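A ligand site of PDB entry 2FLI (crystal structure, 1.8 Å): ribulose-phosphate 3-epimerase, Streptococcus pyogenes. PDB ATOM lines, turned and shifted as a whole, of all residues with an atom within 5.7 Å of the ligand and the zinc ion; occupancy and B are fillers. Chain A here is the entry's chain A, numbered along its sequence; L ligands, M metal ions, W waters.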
ATOM      1  N   SER A   9      18.055   1.253  11.217  1.00  0.00           N
ATOM      2  CA  SER A   9      18.217  -0.156  10.879  1.00  0.00           C
ATOM      3  C   SER A   9      17.000  -0.973  11.297  1.00  0.00           C
ATOM      4  O   SER A   9      16.749  -1.165  12.483  1.00  0.00           O
ATOM      5  CB  SER A   9      19.462  -0.726  11.556  1.00  0.00           C
ATOM      6  OG  SER A   9      19.651  -2.070  11.150  1.00  0.00           O
ATOM      7  N   LEU A  11      16.549  -3.939  11.428  1.00  0.00           N
ATOM      8  CA  LEU A  11      16.878  -5.164  12.148  1.00  0.00           C
ATOM      9  C   LEU A  11      16.539  -4.996  13.623  1.00  0.00           C
ATOM     10  O   LEU A  11      16.353  -5.971  14.338  1.00  0.00           O
ATOM     11  CB  LEU A  11      18.365  -5.482  12.009  1.00  0.00           C
ATOM     12  CG  LEU A  11      18.870  -6.794  12.624  1.00  0.00           C
ATOM     13  CD1 LEU A  11      18.455  -7.967  11.737  1.00  0.00           C
ATOM     14  CD2 LEU A  11      20.387  -6.750  12.779  1.00  0.00           C
ATOM     15  N   ALA A  12      16.474  -3.742  14.075  1.00  0.00           N
ATOM     16  CA  ALA A  12      16.181  -3.450  15.476  1.00  0.00           C
ATOM     17  C   ALA A  12      14.700  -3.159  15.713  1.00  0.00           C
ATOM     18  O   ALA A  12      14.298  -2.834  16.841  1.00  0.00           O
ATOM     19  CB  ALA A  12      17.018  -2.257  15.925  1.00  0.00           C
ATOM     20  N   HIS A  34      17.796   1.125   6.505  1.00  0.00           N
ATOM     21  CA  HIS A  34      18.872   0.157   6.393  1.00  0.00           C
ATOM     22  C   HIS A  34      18.365  -1.264   6.603  1.00  0.00           C
ATOM     23  O   HIS A  34      17.920  -1.608   7.703  1.00  0.00           O
ATOM     24  CB  HIS A  34      19.966   0.445   7.411  1.00  0.00           C
ATOM     25  CG  HIS A  34      21.241  -0.256   7.129  1.00  0.00           C
ATOM     26  ND1 HIS A  34      22.107   0.140   6.130  1.00  0.00           N
ATOM     27  CD2 HIS A  34      21.787  -1.366   7.679  1.00  0.00           C
ATOM     28  CE1 HIS A  34      23.138  -0.689   6.081  1.00  0.00           C
ATOM     29  NE2 HIS A  34      22.966  -1.610   7.009  1.00  0.00           N
ATOM     30  N   ILE A  35      18.443  -2.083   5.564  1.00  0.00           N
ATOM     31  CA  ILE A  35      17.960  -3.457   5.655  1.00  0.00           C
ATOM     32  C   ILE A  35      19.075  -4.499   5.619  1.00  0.00           C
ATOM     33  O   ILE A  35      19.738  -4.680   4.598  1.00  0.00           O
ATOM     34  CB  ILE A  35      16.958  -3.740   4.537  1.00  0.00           C
ATOM     35  CG1 ILE A  35      15.900  -2.635   4.518  1.00  0.00           C
ATOM     36  CG2 ILE A  35      16.308  -5.098   4.751  1.00  0.00           C
ATOM     37  CD1 ILE A  35      15.028  -2.599   3.287  1.00  0.00           C
ATOM     38  N   ASP A  36      19.261  -5.168   6.755  1.00  0.00           N
ATOM     39  CA  ASP A  36      20.292  -6.188   6.897  1.00  0.00           C
ATOM     40  C   ASP A  36      19.815  -7.586   6.520  1.00  0.00           C
ATOM     41  O   ASP A  36      18.920  -8.146   7.153  1.00  0.00           O
ATOM     42  CB  ASP A  36      20.783  -6.223   8.346  1.00  0.00           C
ATOM     43  CG  ASP A  36      21.512  -4.970   8.721  1.00  0.00           C
ATOM     44  OD1 ASP A  36      22.529  -4.693   8.063  1.00  0.00           O
ATOM     45  OD2 ASP A  36      21.079  -4.264   9.656  1.00  0.00           O
ATOM     46  N   MET A  38      20.829 -11.445   6.275  1.00  0.00           N
ATOM     47  CA  MET A  38      21.785 -12.398   6.838  1.00  0.00           C
ATOM     48  C   MET A  38      21.343 -13.824   6.488  1.00  0.00           C
ATOM     49  O   MET A  38      20.170 -14.160   6.644  1.00  0.00           O
ATOM     50  CB  MET A  38      21.838 -12.241   8.371  1.00  0.00           C
ATOM     51  CG  MET A  38      22.369 -10.902   8.858  1.00  0.00           C
ATOM     52  SD  MET A  38      22.172 -10.750  10.656  1.00  0.00           S
ATOM     53  CE  MET A  38      22.162  -8.989  10.875  1.00  0.00           C
ATOM     54  N   HIS A  67      21.892  -4.225   2.845  1.00  0.00           N
ATOM     55  CA  HIS A  67      23.222  -4.672   3.221  1.00  0.00           C
ATOM     56  C   HIS A  67      23.245  -6.193   3.243  1.00  0.00           C
ATOM     57  O   HIS A  67      22.613  -6.820   4.089  1.00  0.00           O
ATOM     58  CB  HIS A  67      23.536  -4.091   4.607  1.00  0.00           C
ATOM     59  CG  HIS A  67      24.853  -4.525   5.160  1.00  0.00           C
ATOM     60  ND1 HIS A  67      25.271  -4.174   6.431  1.00  0.00           N
ATOM     61  CD2 HIS A  67      25.845  -5.292   4.653  1.00  0.00           C
ATOM     62  CE1 HIS A  67      26.449  -4.692   6.672  1.00  0.00           C
ATOM     63  NE2 HIS A  67      26.831  -5.382   5.604  1.00  0.00           N
ATOM     64  N   MET A  69      24.736  -9.504   4.154  1.00  0.00           N
ATOM     65  CA  MET A  69      25.654 -10.282   4.964  1.00  0.00           C
ATOM     66  C   MET A  69      25.360 -11.742   4.631  1.00  0.00           C
ATOM     67  O   MET A  69      24.917 -12.518   5.477  1.00  0.00           O
ATOM     68  CB  MET A  69      25.439  -9.994   6.448  1.00  0.00           C
ATOM     69  CG  MET A  69      25.953  -8.635   6.858  1.00  0.00           C
ATOM     70  SD  MET A  69      25.460  -8.129   8.517  1.00  0.00           S
ATOM     71  CE  MET A  69      23.868  -7.402   8.140  1.00  0.00           C
ATOM     72  N   LEU A 136      30.797   1.432   2.767  1.00  0.00           N
ATOM     73  CA  LEU A 136      30.348   1.236   4.141  1.00  0.00           C
ATOM     74  C   LEU A 136      31.445   0.650   5.011  1.00  0.00           C
ATOM     75  O   LEU A 136      31.982  -0.423   4.713  1.00  0.00           O
ATOM     76  CB  LEU A 136      29.133   0.308   4.173  1.00  0.00           C
ATOM     77  CG  LEU A 136      28.792  -0.308   5.531  1.00  0.00           C
ATOM     78  CD1 LEU A 136      28.599   0.792   6.574  1.00  0.00           C
ATOM     79  CD2 LEU A 136      27.528  -1.144   5.403  1.00  0.00           C
ATOM     80  N   MET A 138      32.099  -0.953   8.494  1.00  0.00           N
ATOM     81  CA  MET A 138      31.439  -1.543   9.660  1.00  0.00           C
ATOM     82  C   MET A 138      32.167  -1.032  10.896  1.00  0.00           C
ATOM     83  O   MET A 138      33.405  -0.981  10.914  1.00  0.00           O
ATOM     84  CB  MET A 138      31.541  -3.077   9.659  1.00  0.00           C
ATOM     85  CG  MET A 138      30.714  -3.788   8.588  1.00  0.00           C
ATOM     86  SD  MET A 138      28.954  -3.437   8.711  1.00  0.00           S
ATOM     87  CE  MET A 138      28.633  -3.721  10.476  1.00  0.00           C
ATOM     88  N   VAL A 140      31.280  -2.345  13.918  1.00  0.00           N
ATOM     89  CA  VAL A 140      31.042  -3.466  14.834  1.00  0.00           C
ATOM     90  C   VAL A 140      31.166  -4.681  13.951  1.00  0.00           C
ATOM     91  O   VAL A 140      31.022  -4.576  12.739  1.00  0.00           O
ATOM     92  CB  VAL A 140      29.604  -3.489  15.457  1.00  0.00           C
ATOM     93  CG1 VAL A 140      29.362  -2.220  16.272  1.00  0.00           C
ATOM     94  CG2 VAL A 140      28.547  -3.671  14.378  1.00  0.00           C
ATOM     95  N   ASN A 141      31.451  -5.841  14.553  1.00  0.00           N
ATOM     96  CA  ASN A 141      31.560  -7.062  13.770  1.00  0.00           C
ATOM     97  C   ASN A 141      30.139  -7.484  13.396  1.00  0.00           C
ATOM     98  O   ASN A 141      29.291  -7.709  14.265  1.00  0.00           O
ATOM     99  CB  ASN A 141      32.269  -8.153  14.580  1.00  0.00           C
ATOM    100  CG  ASN A 141      33.755  -7.896  14.699  1.00  0.00           C
ATOM    101  OD1 ASN A 141      34.498  -8.059  13.727  1.00  0.00           O
ATOM    102  ND2 ASN A 141      34.207  -7.481  15.880  1.00  0.00           N
ATOM    103  N   PRO A 142      29.860  -7.590  12.088  1.00  0.00           N
ATOM    104  CA  PRO A 142      28.547  -7.967  11.530  1.00  0.00           C
ATOM    105  C   PRO A 142      27.870  -9.139  12.232  1.00  0.00           C
ATOM    106  O   PRO A 142      28.525 -10.096  12.616  1.00  0.00           O
ATOM    107  CB  PRO A 142      28.876  -8.295  10.078  1.00  0.00           C
ATOM    108  CG  PRO A 142      30.026  -7.409   9.785  1.00  0.00           C
ATOM    109  CD  PRO A 142      30.873  -7.553  11.019  1.00  0.00           C
ATOM    110  N   GLY A 143      26.552  -9.050  12.383  1.00  0.00           N
ATOM    111  CA  GLY A 143      25.836 -10.149  13.010  1.00  0.00           C
ATOM    112  C   GLY A 143      24.632  -9.778  13.847  1.00  0.00           C
ATOM    113  O   GLY A 143      23.609 -10.460  13.792  1.00  0.00           O
ATOM    114  N   PHE A 144      24.743  -8.708  14.615  1.00  0.00           N
ATOM    115  CA  PHE A 144      23.630  -8.290  15.474  1.00  0.00           C
ATOM    116  C   PHE A 144      23.813  -6.886  16.032  1.00  0.00           C
ATOM    117  O   PHE A 144      24.902  -6.329  16.012  1.00  0.00           O
ATOM    118  CB  PHE A 144      23.432  -9.303  16.605  1.00  0.00           C
ATOM    119  CG  PHE A 144      24.705  -9.753  17.236  1.00  0.00           C
ATOM    120  CD1 PHE A 144      25.270  -9.056  18.304  1.00  0.00           C
ATOM    121  CD2 PHE A 144      25.371 -10.890  16.758  1.00  0.00           C
ATOM    122  CE1 PHE A 144      26.479  -9.476  18.880  1.00  0.00           C
ATOM    123  CE2 PHE A 144      26.568 -11.315  17.313  1.00  0.00           C
ATOM    124  CZ  PHE A 144      27.131 -10.607  18.388  1.00  0.00           C
ATOM    125  N   GLY A 145      22.713  -6.311  16.528  1.00  0.00           N
ATOM    126  CA  GLY A 145      22.773  -4.972  17.072  1.00  0.00           C
ATOM    127  C   GLY A 145      23.222  -4.912  18.517  1.00  0.00           C
ATOM    128  O   GLY A 145      23.574  -5.937  19.102  1.00  0.00           O
ATOM    129  N   GLY A 146      23.215  -3.709  19.080  1.00  0.00           N
ATOM    130  CA  GLY A 146      23.589  -3.516  20.467  1.00  0.00           C
ATOM    131  C   GLY A 146      25.069  -3.743  20.783  1.00  0.00           C
ATOM    132  O   GLY A 146      25.459  -3.639  21.941  1.00  0.00           O
ATOM    133  N   GLN A 147      25.877  -4.033  19.778  1.00  0.00           N
ATOM    134  CA  GLN A 147      27.308  -4.258  19.996  1.00  0.00           C
ATOM    135  C   GLN A 147      28.068  -2.984  20.308  1.00  0.00           C
ATOM    136  O   GLN A 147      27.604  -1.884  20.025  1.00  0.00           O
ATOM    137  CB  GLN A 147      27.946  -4.937  18.776  1.00  0.00           C
ATOM    138  CG  GLN A 147      27.507  -6.368  18.567  1.00  0.00           C
ATOM    139  CD  GLN A 147      28.208  -7.011  17.389  1.00  0.00           C
ATOM    140  OE1 GLN A 147      27.770  -6.875  16.240  1.00  0.00           O
ATOM    141  NE2 GLN A 147      29.303  -7.701  17.662  1.00  0.00           N
ATOM    142  N   ASP A 176      28.296   1.733  10.196  1.00  0.00           N
ATOM    143  CA  ASP A 176      27.233   0.890  10.702  1.00  0.00           C
ATOM    144  C   ASP A 176      27.669   0.032  11.878  1.00  0.00           C
ATOM    145  O   ASP A 176      28.553  -0.828  11.751  1.00  0.00           O
ATOM    146  CB  ASP A 176      26.720   0.019   9.564  1.00  0.00           C
ATOM    147  CG  ASP A 176      25.595  -0.871   9.978  1.00  0.00           C
ATOM    148  OD1 ASP A 176      24.879  -0.544  10.940  1.00  0.00           O
ATOM    149  OD2 ASP A 176      25.415  -1.913   9.317  1.00  0.00           O
ATOM    150  N   GLY A 177      27.064   0.282  13.034  1.00  0.00           N
ATOM    151  CA  GLY A 177      27.391  -0.473  14.229  1.00  0.00           C
ATOM    152  C   GLY A 177      27.734   0.396  15.412  1.00  0.00           C
ATOM    153  O   GLY A 177      28.721   1.140  15.385  1.00  0.00           O
ATOM    154  N   GLY A 178      26.909   0.332  16.449  1.00  0.00           N
ATOM    155  CA  GLY A 178      27.162   1.120  17.637  1.00  0.00           C
ATOM    156  C   GLY A 178      27.134   2.626  17.424  1.00  0.00           C
ATOM    157  O   GLY A 178      27.741   3.366  18.195  1.00  0.00           O
ATOM    158  N   VAL A 179      26.443   3.090  16.388  1.00  0.00           N
ATOM    159  CA  VAL A 179      26.336   4.523  16.146  1.00  0.00           C
ATOM    160  C   VAL A 179      25.201   5.082  17.002  1.00  0.00           C
ATOM    161  O   VAL A 179      24.043   4.680  16.851  1.00  0.00           O
ATOM    162  CB  VAL A 179      26.016   4.844  14.661  1.00  0.00           C
ATOM    163  CG1 VAL A 179      25.917   6.359  14.477  1.00  0.00           C
ATOM    164  CG2 VAL A 179      27.104   4.285  13.763  1.00  0.00           C
ATOM    165  N   VAL A 196      24.086   4.626   9.979  1.00  0.00           N
ATOM    166  CA  VAL A 196      23.121   3.580  10.286  1.00  0.00           C
ATOM    167  C   VAL A 196      23.028   3.408  11.796  1.00  0.00           C
ATOM    168  O   VAL A 196      24.048   3.343  12.478  1.00  0.00           O
ATOM    169  CB  VAL A 196      23.544   2.236   9.670  1.00  0.00           C
ATOM    170  CG1 VAL A 196      22.509   1.155  10.013  1.00  0.00           C
ATOM    171  CG2 VAL A 196      23.678   2.379   8.151  1.00  0.00           C
ATOM    172  N   ALA A 197      21.795   3.352  12.308  1.00  0.00           N
ATOM    173  CA  ALA A 197      21.562   3.200  13.744  1.00  0.00           C
ATOM    174  C   ALA A 197      20.380   2.264  13.987  1.00  0.00           C
ATOM    175  O   ALA A 197      19.290   2.476  13.466  1.00  0.00           O
ATOM    176  CB  ALA A 197      21.293   4.541  14.371  1.00  0.00           C
ATOM    177  N   GLY A 198      20.599   1.237  14.800  1.00  0.00           N
ATOM    178  CA  GLY A 198      19.548   0.296  15.090  1.00  0.00           C
ATOM    179  C   GLY A 198      18.981   0.458  16.491  1.00  0.00           C
ATOM    180  O   GLY A 198      18.026   1.205  16.707  1.00  0.00           O
ATOM    181  N   SER A 199      19.572  -0.244  17.443  1.00  0.00           N
ATOM    182  CA  SER A 199      19.114  -0.218  18.838  1.00  0.00           C
ATOM    183  C   SER A 199      18.942   1.167  19.465  1.00  0.00           C
ATOM    184  O   SER A 199      18.017   1.383  20.243  1.00  0.00           O
ATOM    185  CB  SER A 199      20.051  -1.061  19.702  1.00  0.00           C
ATOM    186  OG  SER A 199      21.367  -0.550  19.662  1.00  0.00           O
ATOM    187  N   TYR A 200      19.835   2.103  19.148  1.00  0.00           N
ATOM    188  CA  TYR A 200      19.732   3.436  19.730  1.00  0.00           C
ATOM    189  C   TYR A 200      18.432   4.143  19.341  1.00  0.00           C
ATOM    190  O   TYR A 200      17.878   4.918  20.118  1.00  0.00           O
ATOM    191  CB  TYR A 200      20.913   4.312  19.329  1.00  0.00           C
ATOM    192  CG  TYR A 200      20.794   5.720  19.843  1.00  0.00           C
ATOM    193  CD1 TYR A 200      20.963   5.994  21.201  1.00  0.00           C
ATOM    194  CD2 TYR A 200      20.473   6.781  18.998  1.00  0.00           C
ATOM    195  CE1 TYR A 200      20.809   7.287  21.697  1.00  0.00           C
ATOM    196  CE2 TYR A 200      20.314   8.065  19.480  1.00  0.00           C
ATOM    197  CZ  TYR A 200      20.484   8.306  20.836  1.00  0.00           C
ATOM    198  OH  TYR A 200      20.315   9.584  21.326  1.00  0.00           O
HETATM  199  C1  LIG L   1      25.028  -5.457  12.182  1.00  0.00           C
HETATM  200  C2  LIG L   1      24.009  -4.764  11.314  1.00  0.00           C
HETATM  201  C3  LIG L   1      23.681  -3.371  11.760  1.00  0.00           C
HETATM  202  C4  LIG L   1      22.869  -3.315  13.013  1.00  0.00           C
HETATM  203  C5  LIG L   1      23.064  -2.054  13.814  1.00  0.00           C
HETATM  204  O1  LIG L   1      25.325  -6.782  11.739  1.00  0.00           O
HETATM  205  O2  LIG L   1      24.517  -4.770   9.969  1.00  0.00           O
HETATM  206  O3  LIG L   1      23.008  -2.619  10.719  1.00  0.00           O
HETATM  207  O4  LIG L   1      21.459  -3.405  12.749  1.00  0.00           O
HETATM  208  O5  LIG L   1      22.807  -2.030  15.206  1.00  0.00           O
HETATM  209  P1  LIG L   1      23.226  -1.049  16.235  1.00  0.00           P
HETATM  210  O6  LIG L   1      22.939   0.385  15.642  1.00  0.00           O
HETATM  211  O7  LIG L   1      24.749  -1.380  16.449  1.00  0.00           O
HETATM  212  O8  LIG L   1      22.273  -1.433  17.483  1.00  0.00           O
HETATM  213 ZN    ZN M   1      24.056  -3.181   7.996  1.00  0.00          ZN
HETATM  214  O   HOH W   1      20.293  -3.177  15.130  1.00  0.00           O
HETATM  215  O   HOH W   2      25.155  -0.992  19.101  1.00  0.00           O
HETATM  216  O   HOH W   3      25.752  -3.907  16.536  1.00  0.00           O
HETATM  217  O   HOH W   4      24.832   1.658  14.273  1.00  0.00           O
HETATM  218  O   HOH W   5      22.523   2.476  17.314  1.00  0.00           O
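The backbone NH (N) of Gly 178 is in hydrogen-bond range of an oxygen (O7) of the ligand (2.8 Å). SD of Met 69 lies within hydrogen-bond range of O1 of the ligand, 3.5 Å away. N of Gly 143 lies within hydrogen-bond range of O1 of the ligand, 2.7 Å away. OG of Ser 199 sits at hydrogen-bond distance from O8 of the ligand (2.5 Å). An oxygen (O8) of the ligand sits at hydrogen-bond distance from the backbone NH of Ser 199, 3.0 Å away. O8 of the ligand sits at hydrogen-bond distance from N of Gly 146. The side-chain hydroxyl (OG) of Ser 9 is in hydrogen-bond range of an oxygen (O4) of the ligand, at 2.8 Å. The backbone NH of Gly 198 sits at hydrogen-bond distance from an oxygen (O6) of the ligand.
The backbone NH (N) of Ser 9 is in hydrogen-bond range of the backbone carbonyl oxygen (O) of Ala 197, 2.8 Å away. OG of Ser 9 is in hydrogen-bond range of OD2 of Asp 36. The backbone carbonyl oxygen (O) of Ile 35 lies within hydrogen-bond range of the backbone NH (N) of His 67. The side-chain amide oxygen (OE1) of Gln 147 lies close to the backbone carbonyl oxygen (O) of Phe 144 (2.9 Å).
Residues that only touch the ligand: Pro 142, Gly 145, Phe 144, Leu 11, Gly 177, Ala 197, Val 196 and Met 38. Hydrophobic or aromatic side chains that line the ligand: Leu 11, His 34, Met 38, His 67, Met 69 and Val 196. 19 residues have an atom within 4 Å of the ligand: Ser 9, Leu 11, His 34, Asp 36, Met 38, His 67, Met 69, Pro 142, Gly 143, Phe 144, Gly 145, Gly 146, Asp 176, Gly 177, Gly 178, Val 196, Ala 197, Gly 198 and Ser 199.
Of the 28 residues printed, 4 come within 4 Å of the zinc ion. The nearest printed residue that does not touch the zinc ion is Met 69 (4.2 Å).
The zinc ion is bound by OD1 of Asp 36 (2.1 Å). NE2 of His 34 is bound to the zinc ion. ND1 of His 67 binds the zinc ion (2.2 Å). The zinc ion is bound by OD2 of Asp 176 (2.3 Å). O2 of the ligand is bound to the zinc ion, 2.6 Å away. The zinc ion has five donor atoms within binding distance.
Water W5 lies within hydrogen-bond range of O6 of the ligand (2.7 Å), O of Val 179 (2.7 Å), N of Tyr 200 (3.3 Å) and N of Gly 198 (3.4 Å). Water W2 lies within hydrogen-bond range of O7 of the ligand (2.7 Å), O of Gln 147 (2.8 Å), N of Gly 146 (3.3 Å) and N of Gly 178 (3.4 Å). Water W3 lies within hydrogen-bond range of O of Phe 144, O7 of the ligand and N of Gln 147.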
